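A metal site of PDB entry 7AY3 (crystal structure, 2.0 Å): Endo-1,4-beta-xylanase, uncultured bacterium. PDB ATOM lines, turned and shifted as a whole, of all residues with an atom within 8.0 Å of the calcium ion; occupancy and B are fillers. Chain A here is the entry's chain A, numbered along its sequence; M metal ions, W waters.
N of Cys 8 sits close to O of Asp 116.
The side-chain carboxylate of Asp 116 lies within salt-bridge range of the guanidinium group of Arg 53 (2.8 Å).
The backbone carbonyl oxygen (O) of Gln 7 lies within hydrogen-bond range of the side-chain hydroxyl (OG) of Ser 10 (2.8 Å).
Of the 16 residues printed, 4 come within 4 Å of the calcium ion.
O of Gly 26 binds the calcium ion, at 2.3 Å.
The side-chain carboxylate (OD1) of Asp 116 is bound to the calcium ion (2.3 Å).
The calcium ion is bound by OE1 of Gln 7 (2.3 Å).
Water W1 binds the calcium ion (2.5 Å).
The calcium ion is bound by OE1 of Glu 9 (2.5 Å).
The calcium ion is bound by OE2 of Glu 9 (2.5 Å).
O of Asp 116 binds the calcium ion (2.6 Å).
The calcium ion has seven donor atoms within binding distance.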
ATOM      1  N   ILE A   5     -17.902 -12.176 -19.476  1.00  0.00           N
ATOM      2  CA  ILE A   5     -17.864 -11.177 -18.424  1.00  0.00           C
ATOM      3  C   ILE A   5     -18.562  -9.927 -18.937  1.00  0.00           C
ATOM      4  O   ILE A   5     -18.232  -9.427 -20.014  1.00  0.00           O
ATOM      5  CB  ILE A   5     -16.410 -10.876 -17.981  1.00  0.00           C
ATOM      6  CG1 ILE A   5     -15.803 -12.116 -17.321  1.00  0.00           C
ATOM      7  CG2 ILE A   5     -16.365  -9.707 -17.007  1.00  0.00           C
ATOM      8  CD1 ILE A   5     -14.437 -11.891 -16.711  1.00  0.00           C
ATOM      9  N   VAL A   6     -19.540  -9.441 -18.165  1.00  0.00           N
ATOM     10  CA  VAL A   6     -20.280  -8.220 -18.469  1.00  0.00           C
ATOM     11  C   VAL A   6     -19.983  -7.204 -17.378  1.00  0.00           C
ATOM     12  O   VAL A   6     -20.322  -7.426 -16.200  1.00  0.00           O
ATOM     13  CB  VAL A   6     -21.798  -8.488 -18.589  1.00  0.00           C
ATOM     14  CG1 VAL A   6     -22.527  -7.243 -19.089  1.00  0.00           C
ATOM     15  CG2 VAL A   6     -22.054  -9.678 -19.512  1.00  0.00           C
ATOM     16  N   GLN A   7     -19.332  -6.112 -17.750  1.00  0.00           N
ATOM     17  CA  GLN A   7     -19.020  -5.063 -16.790  1.00  0.00           C
ATOM     18  C   GLN A   7     -20.298  -4.432 -16.252  1.00  0.00           C
ATOM     19  O   GLN A   7     -21.194  -4.083 -17.020  1.00  0.00           O
ATOM     20  CB  GLN A   7     -18.139  -4.000 -17.444  1.00  0.00           C
ATOM     21  CG  GLN A   7     -16.776  -4.507 -17.863  1.00  0.00           C
ATOM     22  CD  GLN A   7     -16.006  -5.153 -16.719  1.00  0.00           C
ATOM     23  OE1 GLN A   7     -16.128  -4.765 -15.544  1.00  0.00           O
ATOM     24  NE2 GLN A   7     -15.213  -6.154 -17.049  1.00  0.00           N
ATOM     25  N   CYS A   8     -20.373  -4.289 -14.929  1.00  0.00           N
ATOM     26  CA  CYS A   8     -21.588  -3.728 -14.357  1.00  0.00           C
ATOM     27  C   CYS A   8     -21.811  -2.299 -14.826  1.00  0.00           C
ATOM     28  O   CYS A   8     -22.968  -1.862 -14.963  1.00  0.00           O
ATOM     29  CB  CYS A   8     -21.548  -3.814 -12.827  1.00  0.00           C
ATOM     30  SG  CYS A   8     -21.583  -5.503 -12.211  1.00  0.00           S
ATOM     31  N   GLU A   9     -20.734  -1.560 -15.096  1.00  0.00           N
ATOM     32  CA  GLU A   9     -20.883  -0.181 -15.538  1.00  0.00           C
ATOM     33  C   GLU A   9     -21.421  -0.066 -16.963  1.00  0.00           C
ATOM     34  O   GLU A   9     -21.814   1.032 -17.365  1.00  0.00           O
ATOM     35  CB  GLU A   9     -19.561   0.579 -15.410  1.00  0.00           C
ATOM     36  CG  GLU A   9     -18.383  -0.031 -16.190  1.00  0.00           C
ATOM     37  CD  GLU A   9     -17.612  -1.063 -15.372  1.00  0.00           C
ATOM     38  OE1 GLU A   9     -18.223  -1.702 -14.481  1.00  0.00           O
ATOM     39  OE2 GLU A   9     -16.405  -1.221 -15.611  1.00  0.00           O
ATOM     40  N   SER A  10     -21.446  -1.165 -17.712  1.00  0.00           N
ATOM     41  CA  SER A  10     -22.051  -1.180 -19.045  1.00  0.00           C
ATOM     42  C   SER A  10     -23.533  -1.495 -19.039  1.00  0.00           C
ATOM     43  O   SER A  10     -24.185  -1.400 -20.086  1.00  0.00           O
ATOM     44  CB  SER A  10     -21.334  -2.211 -19.935  1.00  0.00           C
ATOM     45  OG  SER A  10     -21.829  -3.516 -19.683  1.00  0.00           O
ATOM     46  N   ILE A  21     -18.771   4.026  -9.886  1.00  0.00           N
ATOM     47  CA  ILE A  21     -17.652   4.236  -8.980  1.00  0.00           C
ATOM     48  C   ILE A  21     -16.359   3.915  -9.715  1.00  0.00           C
ATOM     49  O   ILE A  21     -16.339   3.191 -10.712  1.00  0.00           O
ATOM     50  CB  ILE A  21     -17.760   3.391  -7.702  1.00  0.00           C
ATOM     51  CG1 ILE A  21     -17.791   1.900  -8.065  1.00  0.00           C
ATOM     52  CG2 ILE A  21     -18.994   3.802  -6.908  1.00  0.00           C
ATOM     53  CD1 ILE A  21     -17.941   0.970  -6.874  1.00  0.00           C
ATOM     54  N   PHE A  25     -12.746  -0.493  -7.728  1.00  0.00           N
ATOM     55  CA  PHE A  25     -12.682  -0.910  -9.120  1.00  0.00           C
ATOM     56  C   PHE A  25     -13.603  -0.005  -9.907  1.00  0.00           C
ATOM     57  O   PHE A  25     -14.452   0.680  -9.344  1.00  0.00           O
ATOM     58  CB  PHE A  25     -13.086  -2.381  -9.289  1.00  0.00           C
ATOM     59  CG  PHE A  25     -14.284  -2.790  -8.459  1.00  0.00           C
ATOM     60  CD1 PHE A  25     -15.524  -2.194  -8.648  1.00  0.00           C
ATOM     61  CD2 PHE A  25     -14.158  -3.745  -7.457  1.00  0.00           C
ATOM     62  CE1 PHE A  25     -16.625  -2.561  -7.861  1.00  0.00           C
ATOM     63  CE2 PHE A  25     -15.250  -4.121  -6.666  1.00  0.00           C
ATOM     64  CZ  PHE A  25     -16.479  -3.529  -6.864  1.00  0.00           C
ATOM     65  N   GLY A  26     -13.428  -0.017 -11.231  1.00  0.00           N
ATOM     66  CA  GLY A  26     -14.411   0.592 -12.111  1.00  0.00           C
ATOM     67  C   GLY A  26     -15.692  -0.220 -12.092  1.00  0.00           C
ATOM     68  O   GLY A  26     -15.693  -1.399 -12.492  1.00  0.00           O
ATOM     69  N   GLY A  27     -16.776   0.375 -11.620  1.00  0.00           N
ATOM     70  CA  GLY A  27     -18.011  -0.371 -11.491  1.00  0.00           C
ATOM     71  C   GLY A  27     -19.195   0.491 -11.105  1.00  0.00           C
ATOM     72  O   GLY A  27     -19.261   1.666 -11.497  1.00  0.00           O
ATOM     73  N   VAL A  28     -20.122  -0.076 -10.333  1.00  0.00           N
ATOM     74  CA  VAL A  28     -21.365   0.585  -9.958  1.00  0.00           C
ATOM     75  C   VAL A  28     -21.605   0.383  -8.468  1.00  0.00           C
ATOM     76  O   VAL A  28     -21.271  -0.669  -7.919  1.00  0.00           O
ATOM     77  CB  VAL A  28     -22.541   0.041 -10.790  1.00  0.00           C
ATOM     78  CG1 VAL A  28     -23.821   0.752 -10.434  1.00  0.00           C
ATOM     79  CG2 VAL A  28     -22.251   0.180 -12.274  1.00  0.00           C
ATOM     80  N   ARG A  53     -18.386 -10.169  -9.061  1.00  0.00           N
ATOM     81  CA  ARG A  53     -17.293  -9.567  -8.314  1.00  0.00           C
ATOM     82  C   ARG A  53     -17.757  -8.242  -7.724  1.00  0.00           C
ATOM     83  O   ARG A  53     -18.249  -7.365  -8.449  1.00  0.00           O
ATOM     84  CB  ARG A  53     -16.054  -9.374  -9.190  1.00  0.00           C
ATOM     85  CG  ARG A  53     -14.868  -8.796  -8.406  1.00  0.00           C
ATOM     86  CD  ARG A  53     -13.605  -8.663  -9.252  1.00  0.00           C
ATOM     87  NE  ARG A  53     -12.388  -8.524  -8.450  1.00  0.00           N
ATOM     88  CZ  ARG A  53     -11.622  -7.442  -8.444  1.00  0.00           C
ATOM     89  NH1 ARG A  53     -11.940  -6.398  -9.193  1.00  0.00           N
ATOM     90  NH2 ARG A  53     -10.527  -7.391  -7.685  1.00  0.00           N
ATOM     91  N   ILE A 115     -20.224  -3.135  -7.157  1.00  0.00           N
ATOM     92  CA  ILE A 115     -20.230  -4.294  -8.058  1.00  0.00           C
ATOM     93  C   ILE A 115     -19.417  -3.977  -9.300  1.00  0.00           C
ATOM     94  O   ILE A 115     -19.584  -2.920  -9.929  1.00  0.00           O
ATOM     95  CB  ILE A 115     -21.655  -4.742  -8.415  1.00  0.00           C
ATOM     96  CG1 ILE A 115     -22.506  -3.602  -8.972  1.00  0.00           C
ATOM     97  CG2 ILE A 115     -22.330  -5.337  -7.173  1.00  0.00           C
ATOM     98  CD1 ILE A 115     -23.906  -4.052  -9.390  1.00  0.00           C
ATOM     99  N   ASP A 116     -18.530  -4.904  -9.669  1.00  0.00           N
ATOM    100  CA  ASP A 116     -17.529  -4.717 -10.710  1.00  0.00           C
ATOM    101  C   ASP A 116     -17.969  -5.318 -12.043  1.00  0.00           C
ATOM    102  O   ASP A 116     -18.066  -4.605 -13.040  1.00  0.00           O
ATOM    103  CB  ASP A 116     -16.202  -5.348 -10.253  1.00  0.00           C
ATOM    104  CG  ASP A 116     -15.048  -5.084 -11.224  1.00  0.00           C
ATOM    105  OD1 ASP A 116     -15.240  -4.345 -12.205  1.00  0.00           O
ATOM    106  OD2 ASP A 116     -13.956  -5.603 -10.968  1.00  0.00           O
ATOM    107  N   TYR A 117     -18.234  -6.630 -12.072  1.00  0.00           N
ATOM    108  CA  TYR A 117     -18.645  -7.322 -13.288  1.00  0.00           C
ATOM    109  C   TYR A 117     -19.388  -8.589 -12.910  1.00  0.00           C
ATOM    110  O   TYR A 117     -19.212  -9.127 -11.813  1.00  0.00           O
ATOM    111  CB  TYR A 117     -17.447  -7.669 -14.194  1.00  0.00           C
ATOM    112  CG  TYR A 117     -16.404  -8.557 -13.567  1.00  0.00           C
ATOM    113  CD1 TYR A 117     -16.625  -9.933 -13.385  1.00  0.00           C
ATOM    114  CD2 TYR A 117     -15.190  -8.040 -13.155  1.00  0.00           C
ATOM    115  CE1 TYR A 117     -15.668 -10.742 -12.811  1.00  0.00           C
ATOM    116  CE2 TYR A 117     -14.227  -8.845 -12.587  1.00  0.00           C
ATOM    117  CZ  TYR A 117     -14.465 -10.189 -12.416  1.00  0.00           C
ATOM    118  OH  TYR A 117     -13.492 -10.980 -11.843  1.00  0.00           O
ATOM    119  N   LEU A 118     -20.206  -9.060 -13.839  1.00  0.00           N
ATOM    120  CA  LEU A 118     -20.876 -10.344 -13.725  1.00  0.00           C
ATOM    121  C   LEU A 118     -20.219 -11.327 -14.680  1.00  0.00           C
ATOM    122  O   LEU A 118     -20.067 -11.038 -15.864  1.00  0.00           O
ATOM    123  CB  LEU A 118     -22.370 -10.217 -14.047  1.00  0.00           C
ATOM    124  CG  LEU A 118     -23.153 -11.534 -14.023  1.00  0.00           C
ATOM    125  CD1 LEU A 118     -23.404 -11.993 -12.588  1.00  0.00           C
ATOM    126  CD2 LEU A 118     -24.471 -11.406 -14.791  1.00  0.00           C
HETATM  127 CA    CA M   1     -16.175  -3.103 -13.907  1.00  0.00          CA
HETATM  128  O   HOH W   1     -13.813  -2.745 -14.496  1.00  0.00           O
